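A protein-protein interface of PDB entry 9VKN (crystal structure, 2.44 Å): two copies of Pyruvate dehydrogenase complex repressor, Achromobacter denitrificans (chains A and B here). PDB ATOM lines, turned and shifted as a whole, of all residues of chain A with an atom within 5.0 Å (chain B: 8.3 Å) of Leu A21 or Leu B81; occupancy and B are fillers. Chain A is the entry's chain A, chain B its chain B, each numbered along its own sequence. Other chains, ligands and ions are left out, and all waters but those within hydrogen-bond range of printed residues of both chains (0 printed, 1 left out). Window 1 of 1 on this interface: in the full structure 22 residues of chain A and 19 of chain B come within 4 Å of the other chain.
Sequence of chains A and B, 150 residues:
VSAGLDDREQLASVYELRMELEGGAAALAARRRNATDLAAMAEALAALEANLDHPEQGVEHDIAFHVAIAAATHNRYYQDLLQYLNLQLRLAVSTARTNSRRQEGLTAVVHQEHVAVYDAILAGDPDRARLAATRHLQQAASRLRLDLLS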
ATOM      1  N   LEU A  17     -26.649  29.157  21.227  1.00  0.00           N
ATOM      2  CA  LEU A  17     -25.598  28.258  20.763  1.00  0.00           C
ATOM      3  C   LEU A  17     -26.172  26.922  20.285  1.00  0.00           C
ATOM      4  O   LEU A  17     -25.733  26.377  19.265  1.00  0.00           O
ATOM      5  CB  LEU A  17     -24.586  28.057  21.884  1.00  0.00           C
ATOM      6  CG  LEU A  17     -23.520  27.028  21.551  1.00  0.00           C
ATOM      7  CD1 LEU A  17     -22.582  27.617  20.495  1.00  0.00           C
ATOM      8  CD2 LEU A  17     -22.778  26.639  22.802  1.00  0.00           C
ATOM      9  N   ARG A  18     -27.154  26.371  21.007  1.00  0.00           N
ATOM     10  CA  ARG A  18     -27.718  25.088  20.596  1.00  0.00           C
ATOM     11  C   ARG A  18     -28.274  25.157  19.177  1.00  0.00           C
ATOM     12  O   ARG A  18     -28.088  24.228  18.383  1.00  0.00           O
ATOM     13  CB  ARG A  18     -28.797  24.646  21.583  1.00  0.00           C
ATOM     14  CG  ARG A  18     -28.240  24.174  22.908  1.00  0.00           C
ATOM     15  CD  ARG A  18     -29.351  23.723  23.819  1.00  0.00           C
ATOM     16  NE  ARG A  18     -29.927  22.463  23.378  1.00  0.00           N
ATOM     17  CZ  ARG A  18     -31.037  21.947  23.895  1.00  0.00           C
ATOM     18  NH1 ARG A  18     -31.666  22.595  24.867  1.00  0.00           N
ATOM     19  NH2 ARG A  18     -31.509  20.791  23.454  1.00  0.00           N
ATOM     20  N   MET A  19     -28.919  26.267  18.828  1.00  0.00           N
ATOM     21  CA  MET A  19     -29.566  26.360  17.527  1.00  0.00           C
ATOM     22  C   MET A  19     -28.570  26.149  16.386  1.00  0.00           C
ATOM     23  O   MET A  19     -28.879  25.462  15.404  1.00  0.00           O
ATOM     24  CB  MET A  19     -30.272  27.704  17.408  1.00  0.00           C
ATOM     25  CG  MET A  19     -31.770  27.588  17.481  1.00  0.00           C
ATOM     26  SD  MET A  19     -32.553  29.201  17.599  1.00  0.00           S
ATOM     27  CE  MET A  19     -32.286  29.752  15.909  1.00  0.00           C
ATOM     28  N   GLU A  20     -27.373  26.732  16.495  1.00  0.00           N
ATOM     29  CA  GLU A  20     -26.309  26.454  15.530  1.00  0.00           C
ATOM     30  C   GLU A  20     -25.771  25.039  15.676  1.00  0.00           C
ATOM     31  O   GLU A  20     -25.799  24.240  14.730  1.00  0.00           O
ATOM     32  CB  GLU A  20     -25.172  27.456  15.708  1.00  0.00           C
ATOM     33  CG  GLU A  20     -25.666  28.877  15.660  1.00  0.00           C
ATOM     34  CD  GLU A  20     -26.064  29.307  14.251  1.00  0.00           C
ATOM     35  OE1 GLU A  20     -25.794  28.553  13.279  1.00  0.00           O
ATOM     36  OE2 GLU A  20     -26.650  30.407  14.117  1.00  0.00           O
ATOM     37  N   LEU A  21     -25.248  24.721  16.855  1.00  0.00           N
ATOM     38  CA  LEU A  21     -24.549  23.455  17.037  1.00  0.00           C
ATOM     39  C   LEU A  21     -25.462  22.277  16.731  1.00  0.00           C
ATOM     40  O   LEU A  21     -25.084  21.351  16.002  1.00  0.00           O
ATOM     41  CB  LEU A  21     -24.017  23.371  18.462  1.00  0.00           C
ATOM     42  CG  LEU A  21     -22.537  23.635  18.676  1.00  0.00           C
ATOM     43  CD1 LEU A  21     -22.292  23.917  20.148  1.00  0.00           C
ATOM     44  CD2 LEU A  21     -21.746  22.404  18.249  1.00  0.00           C
ATOM     45  N   GLU A  22     -26.687  22.309  17.248  1.00  0.00           N
ATOM     46  CA  GLU A  22     -27.565  21.166  17.035  1.00  0.00           C
ATOM     47  C   GLU A  22     -28.224  21.192  15.663  1.00  0.00           C
ATOM     48  O   GLU A  22     -28.570  20.125  15.137  1.00  0.00           O
ATOM     49  CB  GLU A  22     -28.590  21.090  18.166  1.00  0.00           C
ATOM     50  CG  GLU A  22     -27.906  20.714  19.479  1.00  0.00           C
ATOM     51  CD  GLU A  22     -28.862  20.573  20.636  1.00  0.00           C
ATOM     52  OE1 GLU A  22     -30.068  20.415  20.397  1.00  0.00           O
ATOM     53  OE2 GLU A  22     -28.404  20.620  21.789  1.00  0.00           O
ATOM     54  N   GLY A  23     -28.385  22.371  15.053  1.00  0.00           N
ATOM     55  CA  GLY A  23     -28.784  22.404  13.655  1.00  0.00           C
ATOM     56  C   GLY A  23     -27.758  21.729  12.762  1.00  0.00           C
ATOM     57  O   GLY A  23     -28.093  20.883  11.927  1.00  0.00           O
ATOM     58  N   GLY A  24     -26.484  22.074  12.948  1.00  0.00           N
ATOM     59  CA  GLY A  24     -25.441  21.458  12.145  1.00  0.00           C
ATOM     60  C   GLY A  24     -25.349  19.966  12.385  1.00  0.00           C
ATOM     61  O   GLY A  24     -25.283  19.173  11.439  1.00  0.00           O
ATOM     62  N   ALA A  25     -25.384  19.564  13.662  1.00  0.00           N
ATOM     63  CA  ALA A  25     -25.274  18.153  14.004  1.00  0.00           C
ATOM     64  C   ALA A  25     -26.388  17.341  13.366  1.00  0.00           C
ATOM     65  O   ALA A  25     -26.151  16.217  12.902  1.00  0.00           O
ATOM     66  CB  ALA A  25     -25.285  17.963  15.523  1.00  0.00           C
ATOM     67  N   TYR A  78     -17.750  16.826  17.896  1.00  0.00           N
ATOM     68  CA  TYR A  78     -19.124  17.216  18.271  1.00  0.00           C
ATOM     69  C   TYR A  78     -19.553  16.572  19.578  1.00  0.00           C
ATOM     70  O   TYR A  78     -20.090  17.286  20.391  1.00  0.00           O
ATOM     71  CB  TYR A  78     -20.136  16.761  17.226  1.00  0.00           C
ATOM     72  CG  TYR A  78     -20.611  17.802  16.253  1.00  0.00           C
ATOM     73  CD1 TYR A  78     -21.713  18.568  16.512  1.00  0.00           C
ATOM     74  CD2 TYR A  78     -19.984  17.980  15.044  1.00  0.00           C
ATOM     75  CE1 TYR A  78     -22.158  19.507  15.605  1.00  0.00           C
ATOM     76  CE2 TYR A  78     -20.419  18.905  14.123  1.00  0.00           C
ATOM     77  CZ  TYR A  78     -21.517  19.673  14.404  1.00  0.00           C
ATOM     78  OH  TYR A  78     -21.963  20.580  13.507  1.00  0.00           O
ATOM     79  N   LEU A  81     -18.069  18.436  22.589  1.00  0.00           N
ATOM     80  CA  LEU A  81     -18.615  19.780  22.894  1.00  0.00           C
ATOM     81  C   LEU A  81     -19.899  19.617  23.679  1.00  0.00           C
ATOM     82  O   LEU A  81     -20.056  20.294  24.635  1.00  0.00           O
ATOM     83  CB  LEU A  81     -18.872  20.549  21.600  1.00  0.00           C
ATOM     84  CG  LEU A  81     -17.625  21.050  20.894  1.00  0.00           C
ATOM     85  CD1 LEU A  81     -17.967  22.100  19.867  1.00  0.00           C
ATOM     86  CD2 LEU A  81     -16.650  21.604  21.883  1.00  0.00           C
ATOM     87  N   TYR A  84     -18.859  18.686  27.129  1.00  0.00           N
ATOM     88  CA  TYR A  84     -18.278  19.861  27.783  1.00  0.00           C
ATOM     89  C   TYR A  84     -19.350  20.845  28.259  1.00  0.00           C
ATOM     90  O   TYR A  84     -19.125  21.599  29.218  1.00  0.00           O
ATOM     91  CB  TYR A  84     -17.312  20.546  26.809  1.00  0.00           C
ATOM     92  CG  TYR A  84     -16.630  21.821  27.277  1.00  0.00           C
ATOM     93  CD1 TYR A  84     -15.451  21.784  28.017  1.00  0.00           C
ATOM     94  CD2 TYR A  84     -17.142  23.053  26.951  1.00  0.00           C
ATOM     95  CE1 TYR A  84     -14.820  22.959  28.421  1.00  0.00           C
ATOM     96  CE2 TYR A  84     -16.528  24.218  27.332  1.00  0.00           C
ATOM     97  CZ  TYR A  84     -15.369  24.178  28.068  1.00  0.00           C
ATOM     98  OH  TYR A  84     -14.783  25.377  28.445  1.00  0.00           O
ATOM     99  N   LEU A  85     -20.517  20.851  27.609  1.00  0.00           N
ATOM    100  CA  LEU A  85     -21.603  21.761  27.945  1.00  0.00           C
ATOM    101  C   LEU A  85     -22.729  21.080  28.716  1.00  0.00           C
ATOM    102  O   LEU A  85     -23.820  21.650  28.822  1.00  0.00           O
ATOM    103  CB  LEU A  85     -22.158  22.411  26.678  1.00  0.00           C
ATOM    104  CG  LEU A  85     -21.191  23.356  25.928  1.00  0.00           C
ATOM    105  CD1 LEU A  85     -21.498  23.405  24.414  1.00  0.00           C
ATOM    106  CD2 LEU A  85     -21.179  24.752  26.526  1.00  0.00           C
ATOM    107  N   LEU B  17     -16.327  20.725  11.978  1.00  0.00           N
ATOM    108  CA  LEU B  17     -16.909  21.358  13.157  1.00  0.00           C
ATOM    109  C   LEU B  17     -16.794  22.880  13.096  1.00  0.00           C
ATOM    110  O   LEU B  17     -17.753  23.585  13.429  1.00  0.00           O
ATOM    111  CB  LEU B  17     -16.236  20.822  14.420  1.00  0.00           C
ATOM    112  CG  LEU B  17     -16.715  21.518  15.688  1.00  0.00           C
ATOM    113  CD1 LEU B  17     -18.239  21.299  15.884  1.00  0.00           C
ATOM    114  CD2 LEU B  17     -15.923  21.024  16.877  1.00  0.00           C
ATOM    115  N   GLU B  20     -19.628  24.772  11.236  1.00  0.00           N
ATOM    116  CA  GLU B  20     -20.870  25.080  11.926  1.00  0.00           C
ATOM    117  C   GLU B  20     -20.636  26.083  13.048  1.00  0.00           C
ATOM    118  O   GLU B  20     -21.373  27.063  13.168  1.00  0.00           O
ATOM    119  CB  GLU B  20     -21.510  23.791  12.438  1.00  0.00           C
ATOM    120  CG  GLU B  20     -21.707  22.767  11.316  1.00  0.00           C
ATOM    121  CD  GLU B  20     -22.894  23.106  10.428  1.00  0.00           C
ATOM    122  OE1 GLU B  20     -23.710  23.964  10.837  1.00  0.00           O
ATOM    123  OE2 GLU B  20     -23.017  22.512   9.325  1.00  0.00           O
ATOM    124  N   LEU B  21     -19.597  25.875  13.858  1.00  0.00           N
ATOM    125  CA  LEU B  21     -19.333  26.797  14.958  1.00  0.00           C
ATOM    126  C   LEU B  21     -19.092  28.219  14.465  1.00  0.00           C
ATOM    127  O   LEU B  21     -19.611  29.180  15.040  1.00  0.00           O
ATOM    128  CB  LEU B  21     -18.125  26.328  15.756  1.00  0.00           C
ATOM    129  CG  LEU B  21     -18.480  25.825  17.139  1.00  0.00           C
ATOM    130  CD1 LEU B  21     -19.208  24.528  16.964  1.00  0.00           C
ATOM    131  CD2 LEU B  21     -17.206  25.636  17.952  1.00  0.00           C
ATOM    132  N   GLU B  22     -18.273  28.379  13.424  1.00  0.00           N
ATOM    133  CA  GLU B  22     -17.856  29.718  13.011  1.00  0.00           C
ATOM    134  C   GLU B  22     -18.874  30.382  12.092  1.00  0.00           C
ATOM    135  O   GLU B  22     -19.065  31.600  12.166  1.00  0.00           O
ATOM    136  CB  GLU B  22     -16.475  29.651  12.361  1.00  0.00           C
ATOM    137  CG  GLU B  22     -15.451  28.939  13.240  1.00  0.00           C
ATOM    138  CD  GLU B  22     -14.008  29.262  12.868  1.00  0.00           C
ATOM    139  OE1 GLU B  22     -13.789  30.166  12.025  1.00  0.00           O
ATOM    140  OE2 GLU B  22     -13.085  28.602  13.404  1.00  0.00           O
ATOM    141  N   GLY B  24     -22.137  30.054  12.481  1.00  0.00           N
ATOM    142  CA  GLY B  24     -23.088  30.579  13.443  1.00  0.00           C
ATOM    143  C   GLY B  24     -22.546  31.768  14.209  1.00  0.00           C
ATOM    144  O   GLY B  24     -23.254  32.758  14.399  1.00  0.00           O
ATOM    145  N   VAL B  67     -11.015  34.162  16.863  1.00  0.00           N
ATOM    146  CA  VAL B  67     -11.402  34.367  18.260  1.00  0.00           C
ATOM    147  C   VAL B  67     -12.121  35.709  18.438  1.00  0.00           C
ATOM    148  O   VAL B  67     -13.107  35.810  19.182  1.00  0.00           O
ATOM    149  CB  VAL B  67     -10.172  34.238  19.180  1.00  0.00           C
ATOM    150  CG1 VAL B  67     -10.440  34.876  20.534  1.00  0.00           C
ATOM    151  CG2 VAL B  67      -9.808  32.766  19.367  1.00  0.00           C
ATOM    152  N   ALA B  70     -15.668  35.445  17.518  1.00  0.00           N
ATOM    153  CA  ALA B  70     -16.392  34.760  18.582  1.00  0.00           C
ATOM    154  C   ALA B  70     -16.690  35.701  19.753  1.00  0.00           C
ATOM    155  O   ALA B  70     -17.808  35.706  20.282  1.00  0.00           O
ATOM    156  CB  ALA B  70     -15.591  33.539  19.036  1.00  0.00           C
ATOM    157  N   ASN B  75     -21.790  36.066  23.294  1.00  0.00           N
ATOM    158  CA  ASN B  75     -22.330  34.859  23.897  1.00  0.00           C
ATOM    159  C   ASN B  75     -21.132  34.084  24.419  1.00  0.00           C
ATOM    160  O   ASN B  75     -20.281  33.665  23.631  1.00  0.00           O
ATOM    161  CB  ASN B  75     -23.133  34.068  22.863  1.00  0.00           C
ATOM    162  CG  ASN B  75     -23.543  32.687  23.342  1.00  0.00           C
ATOM    163  OD1 ASN B  75     -22.832  32.020  24.109  1.00  0.00           O
ATOM    164  ND2 ASN B  75     -24.687  32.227  22.844  1.00  0.00           N
ATOM    165  N   ARG B  76     -21.086  33.878  25.741  1.00  0.00           N
ATOM    166  CA  ARG B  76     -19.872  33.414  26.410  1.00  0.00           C
ATOM    167  C   ARG B  76     -19.511  31.988  26.023  1.00  0.00           C
ATOM    168  O   ARG B  76     -18.356  31.574  26.176  1.00  0.00           O
ATOM    169  CB  ARG B  76     -20.040  33.523  27.931  1.00  0.00           C
ATOM    170  N   TYR B  77     -20.470  31.223  25.511  1.00  0.00           N
ATOM    171  CA  TYR B  77     -20.180  29.834  25.179  1.00  0.00           C
ATOM    172  C   TYR B  77     -19.481  29.705  23.822  1.00  0.00           C
ATOM    173  O   TYR B  77     -18.749  28.735  23.582  1.00  0.00           O
ATOM    174  CB  TYR B  77     -21.475  29.033  25.240  1.00  0.00           C
ATOM    175  CG  TYR B  77     -22.144  29.139  26.600  1.00  0.00           C
ATOM    176  CD1 TYR B  77     -21.456  28.781  27.741  1.00  0.00           C
ATOM    177  CD2 TYR B  77     -23.439  29.625  26.746  1.00  0.00           C
ATOM    178  CE1 TYR B  77     -22.032  28.860  28.999  1.00  0.00           C
ATOM    179  CE2 TYR B  77     -24.038  29.713  28.020  1.00  0.00           C
ATOM    180  CZ  TYR B  77     -23.313  29.323  29.143  1.00  0.00           C
ATOM    181  OH  TYR B  77     -23.837  29.388  30.424  1.00  0.00           O
ATOM    182  N   TYR B  78     -19.650  30.689  22.932  1.00  0.00           N
ATOM    183  CA  TYR B  78     -18.852  30.677  21.705  1.00  0.00           C
ATOM    184  C   TYR B  78     -17.370  30.851  22.013  1.00  0.00           C
ATOM    185  O   TYR B  78     -16.517  30.182  21.415  1.00  0.00           O
ATOM    186  CB  TYR B  78     -19.325  31.763  20.738  1.00  0.00           C
ATOM    187  CG  TYR B  78     -20.456  31.328  19.844  1.00  0.00           C
ATOM    188  CD1 TYR B  78     -20.211  30.536  18.717  1.00  0.00           C
ATOM    189  CD2 TYR B  78     -21.769  31.706  20.119  1.00  0.00           C
ATOM    190  CE1 TYR B  78     -21.242  30.130  17.882  1.00  0.00           C
ATOM    191  CE2 TYR B  78     -22.815  31.297  19.292  1.00  0.00           C
ATOM    192  CZ  TYR B  78     -22.536  30.524  18.179  1.00  0.00           C
ATOM    193  OH  TYR B  78     -23.560  30.130  17.381  1.00  0.00           O
ATOM    194  N   GLN B  79     -17.038  31.739  22.943  1.00  0.00           N
ATOM    195  CA  GLN B  79     -15.632  31.925  23.275  1.00  0.00           C
ATOM    196  C   GLN B  79     -15.075  30.704  23.996  1.00  0.00           C
ATOM    197  O   GLN B  79     -13.956  30.265  23.698  1.00  0.00           O
ATOM    198  CB  GLN B  79     -15.473  33.197  24.107  1.00  0.00           C
ATOM    199  CG  GLN B  79     -16.481  34.280  23.683  1.00  0.00           C
ATOM    200  CD  GLN B  79     -16.223  35.626  24.333  1.00  0.00           C
ATOM    201  OE1 GLN B  79     -15.062  36.038  24.518  1.00  0.00           O
ATOM    202  NE2 GLN B  79     -17.309  36.331  24.681  1.00  0.00           N
ATOM    203  N   ASP B  80     -15.859  30.120  24.914  1.00  0.00           N
ATOM    204  CA  ASP B  80     -15.397  28.955  25.671  1.00  0.00           C
ATOM    205  C   ASP B  80     -15.072  27.785  24.765  1.00  0.00           C
ATOM    206  O   ASP B  80     -14.056  27.110  24.965  1.00  0.00           O
ATOM    207  CB  ASP B  80     -16.442  28.514  26.700  1.00  0.00           C
ATOM    208  CG  ASP B  80     -16.686  29.552  27.766  1.00  0.00           C
ATOM    209  OD1 ASP B  80     -16.076  30.640  27.685  1.00  0.00           O
ATOM    210  OD2 ASP B  80     -17.503  29.276  28.676  1.00  0.00           O
ATOM    211  N   LEU B  81     -15.935  27.500  23.789  1.00  0.00           N
ATOM    212  CA  LEU B  81     -15.706  26.350  22.923  1.00  0.00           C
ATOM    213  C   LEU B  81     -14.497  26.559  22.027  1.00  0.00           C
ATOM    214  O   LEU B  81     -13.754  25.610  21.744  1.00  0.00           O
ATOM    215  CB  LEU B  81     -16.958  26.036  22.100  1.00  0.00           C
ATOM    216  CG  LEU B  81     -18.152  25.616  22.958  1.00  0.00           C
ATOM    217  CD1 LEU B  81     -19.338  25.312  22.093  1.00  0.00           C
ATOM    218  CD2 LEU B  81     -17.782  24.419  23.835  1.00  0.00           C
ATOM    219  N   LEU B  82     -14.287  27.794  21.563  1.00  0.00           N
ATOM    220  CA  LEU B  82     -13.116  28.070  20.739  1.00  0.00           C
ATOM    221  C   LEU B  82     -11.848  28.015  21.573  1.00  0.00           C
ATOM    222  O   LEU B  82     -10.809  27.535  21.102  1.00  0.00           O
ATOM    223  CB  LEU B  82     -13.244  29.430  20.048  1.00  0.00           C
ATOM    224  CG  LEU B  82     -13.649  29.355  18.572  1.00  0.00           C
ATOM    225  CD1 LEU B  82     -15.131  28.993  18.450  1.00  0.00           C
ATOM    226  CD2 LEU B  82     -13.337  30.652  17.829  1.00  0.00           C
ATOM    227  N   GLN B  83     -11.910  28.498  22.819  1.00  0.00           N
ATOM    228  CA  GLN B  83     -10.779  28.311  23.722  1.00  0.00           C
ATOM    229  C   GLN B  83     -10.588  26.838  24.032  1.00  0.00           C
ATOM    230  O   GLN B  83      -9.457  26.346  24.107  1.00  0.00           O
ATOM    231  CB  GLN B  83     -10.985  29.108  25.010  1.00  0.00           C
ATOM    232  CG  GLN B  83      -9.775  29.050  25.936  1.00  0.00           C
ATOM    233  CD  GLN B  83      -8.635  29.960  25.477  1.00  0.00           C
ATOM    234  OE1 GLN B  83      -8.158  29.862  24.340  1.00  0.00           O
ATOM    235  NE2 GLN B  83      -8.188  30.843  26.368  1.00  0.00           N
ATOM    236  N   TYR B  84     -11.698  26.118  24.165  1.00  0.00           N
ATOM    237  CA  TYR B  84     -11.648  24.696  24.458  1.00  0.00           C
ATOM    238  C   TYR B  84     -10.986  23.920  23.329  1.00  0.00           C
ATOM    239  O   TYR B  84     -10.310  22.910  23.570  1.00  0.00           O
ATOM    240  CB  TYR B  84     -13.068  24.180  24.703  1.00  0.00           C
ATOM    241  CG  TYR B  84     -13.102  22.697  24.917  1.00  0.00           C
ATOM    242  CD1 TYR B  84     -12.534  22.143  26.058  1.00  0.00           C
ATOM    243  CD2 TYR B  84     -13.669  21.847  23.990  1.00  0.00           C
ATOM    244  CE1 TYR B  84     -12.535  20.781  26.277  1.00  0.00           C
ATOM    245  CE2 TYR B  84     -13.681  20.474  24.199  1.00  0.00           C
ATOM    246  CZ  TYR B  84     -13.116  19.954  25.354  1.00  0.00           C
ATOM    247  OH  TYR B  84     -13.112  18.601  25.582  1.00  0.00           O
ATOM    248  N   LEU B  85     -11.193  24.364  22.087  1.00  0.00           N
ATOM    249  CA  LEU B  85     -10.684  23.686  20.902  1.00  0.00           C
ATOM    250  C   LEU B  85      -9.417  24.330  20.361  1.00  0.00           C
ATOM    251  O   LEU B  85      -9.036  24.051  19.217  1.00  0.00           O
ATOM    252  CB  LEU B  85     -11.750  23.674  19.809  1.00  0.00           C
ATOM    253  CG  LEU B  85     -13.004  22.843  20.022  1.00  0.00           C
ATOM    254  CD1 LEU B  85     -14.087  23.325  19.074  1.00  0.00           C
ATOM    255  CD2 LEU B  85     -12.697  21.377  19.793  1.00  0.00           C
ATOM    256  N   ASN B  86      -8.776  25.197  21.148  1.00  0.00           N
ATOM    257  CA  ASN B  86      -7.626  25.958  20.664  1.00  0.00           C
ATOM    258  C   ASN B  86      -6.548  25.071  20.061  1.00  0.00           C
ATOM    259  O   ASN B  86      -5.912  25.448  19.070  1.00  0.00           O
ATOM    260  CB  ASN B  86      -7.026  26.787  21.794  1.00  0.00           C
ATOM    261  CG  ASN B  86      -5.831  27.593  21.339  1.00  0.00           C
ATOM    262  OD1 ASN B  86      -4.702  27.362  21.770  1.00  0.00           O
ATOM    263  ND2 ASN B  86      -6.074  28.536  20.435  1.00  0.00           N
ATOM    264  N   LEU B  87      -6.307  23.900  20.658  1.00  0.00           N
ATOM    265  CA  LEU B  87      -5.255  23.022  20.153  1.00  0.00           C
ATOM    266  C   LEU B  87      -5.592  22.519  18.758  1.00  0.00           C
ATOM    267  O   LEU B  87      -4.722  22.472  17.879  1.00  0.00           O
ATOM    268  CB  LEU B  87      -5.037  21.840  21.097  1.00  0.00           C
ATOM    269  CG  LEU B  87      -4.235  20.693  20.478  1.00  0.00           C
ATOM    270  CD1 LEU B  87      -2.775  21.088  20.353  1.00  0.00           C
ATOM    271  CD2 LEU B  87      -4.368  19.386  21.251  1.00  0.00           C
ATOM    272  N   GLN B  88      -6.850  22.119  18.552  1.00  0.00           N
ATOM    273  CA  GLN B  88      -7.299  21.709  17.230  1.00  0.00           C
ATOM    274  C   GLN B  88      -7.223  22.870  16.250  1.00  0.00           C
ATOM    275  O   GLN B  88      -6.831  22.689  15.089  1.00  0.00           O
ATOM    276  CB  GLN B  88      -8.721  21.160  17.318  1.00  0.00           C
ATOM    277  CG  GLN B  88      -8.826  19.758  17.920  1.00  0.00           C
ATOM    278  CD  GLN B  88      -8.457  19.712  19.398  1.00  0.00           C
ATOM    279  OE1 GLN B  88      -8.639  20.686  20.138  1.00  0.00           O
ATOM    280  NE2 GLN B  88      -7.918  18.574  19.831  1.00  0.00           N
ATOM    281  N   LEU B  89      -7.573  24.076  16.699  1.00  0.00           N
ATOM    282  CA  LEU B  89      -7.473  25.230  15.815  1.00  0.00           C
ATOM    283  C   LEU B  89      -6.034  25.460  15.374  1.00  0.00           C
ATOM    284  O   LEU B  89      -5.766  25.635  14.183  1.00  0.00           O
ATOM    285  CB  LEU B  89      -8.038  26.474  16.493  1.00  0.00           C
ATOM    286  CG  LEU B  89      -9.341  26.937  15.849  1.00  0.00           C
ATOM    287  CD1 LEU B  89     -10.379  25.808  15.865  1.00  0.00           C
ATOM    288  CD2 LEU B  89      -9.882  28.157  16.561  1.00  0.00           C
ATOM    289  N   ARG B 130     -22.384  34.536   7.730  1.00  0.00           N
ATOM    290  CA  ARG B 130     -22.315  33.081   7.858  1.00  0.00           C
ATOM    291  C   ARG B 130     -21.730  32.446   6.602  1.00  0.00           C
ATOM    292  O   ARG B 130     -20.905  31.528   6.689  1.00  0.00           O
ATOM    293  CB  ARG B 130     -23.710  32.510   8.164  1.00  0.00           C
ATOM    294  CG  ARG B 130     -23.870  31.006   7.914  1.00  0.00           C
ATOM    295  CD  ARG B 130     -25.355  30.592   7.797  1.00  0.00           C
ATOM    296  NE  ARG B 130     -26.168  31.087   8.909  1.00  0.00           N
ATOM    297  CZ  ARG B 130     -26.051  30.663  10.169  1.00  0.00           C
ATOM    298  NH1 ARG B 130     -26.827  31.174  11.114  1.00  0.00           N
ATOM    299  NH2 ARG B 130     -25.161  29.724  10.492  1.00  0.00           N
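The guanidinium group of Arg B130 lies within salt-bridge range of the side-chain carboxylate of Glu A20 (3.1 Å).
N of Tyr B77 sits at hydrogen-bond distance from OD1 of Asn B75 (2.9 Å).
N of Leu A17 touches ND2 of Asn B75, at 3.99 Å.
Tyr B77 touches Leu A17.
Leu A17 touches Leu B81.
Gly B24 touches Glu A20 (CA to CD, 3.3 Å).
Leu A21 touches Leu B81 (CD1 to CD1, 3.8 Å).
Glu B20 touches Tyr A78.
CD2 of Leu B17 touches CD1 of Leu A81 (3.8 Å).
Leu B81 touches Leu A81 (CD2 to CD2, 3.6 Å).
Leu A81 touches Tyr B84.
CD1 of Leu A85 touches CD1 of Leu B81, at 3.7 Å.
Leu A21 touches just these residues of chain B: Leu B21 and Leu B81.
Glu A22 touches none of the printed residues of chain B.
Of the printed residues of chain A, Asn B75 touches Leu A17 (3.99 Å).
Of the printed residues of chain A, Tyr B78 touches Leu A17 (3.7 Å) and Glu A20 (3.0 Å).
Of the printed residues of chain A, Asp B80 touches Tyr A84 (3.95 Å).
Of chain A, only Leu A17, Leu A21, Leu A81, Tyr A84 and Leu A85 come within 4 Å of Leu B81.
Leu B89 touches none of the printed residues of chain A.
Printed residues of chain A within 4 Å of Arg B130: Glu A20 (3.1 Å).
The nearest residue of chain B that does not touch Leu A21 is Leu B17 (4.4 Å).
The nearest printed residue of chain A that does not touch Leu B81 is Arg A18 (8.0 Å).
The nearest printed residue of chain B that does not touch Tyr A84 is Gln B83 (6.3 Å).
Hydrophobic or aromatic side chains of chain B within 4 Å of the printed part of chain A: Leu B17, Leu B21, Tyr B77, Tyr B78, Leu B81 and Tyr B84.
Along chain B the printed residues that touch a printed residue of chain A span positions 17 to 130.
Of the 13 printed residues of chain A, 8 touch a printed residue of chain B.
Printed residues of chain A that touch a printed residue of chain B: Leu A17, Glu A20, Leu A21, Gly A24, Tyr A78, Leu A81, Tyr A84 and Leu A85.
Hydrophobic or aromatic side chains of chain A within 4 Å of the printed part of chain B: Leu A17, Leu A21, Tyr A78, Leu A81, Tyr A84 and Leu A85.
Among the printed residues, Asp or Glu carboxylates within 4 Å of a Lys or Arg side-chain nitrogen of the other chain: Glu A20 with Arg B130 (3.1 Å).
Leu A17 touches Tyr B78, and with the chains exchanged Tyr A78 touches Leu B17.
Glu A20 touches Gly B24, and with the chains exchanged Gly A24 touches Glu B20.
Glu A20 touches Tyr B78, and with the chains exchanged Tyr A78 touches Glu B20.
Leu A85 touches Leu B81, but with the chains exchanged Leu A81 does not touch Leu B85 (4.1 Å).
Of the 20 pairs that touch across the chains among the printed residues, 15 have their exchanged pair printed and touching as well.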
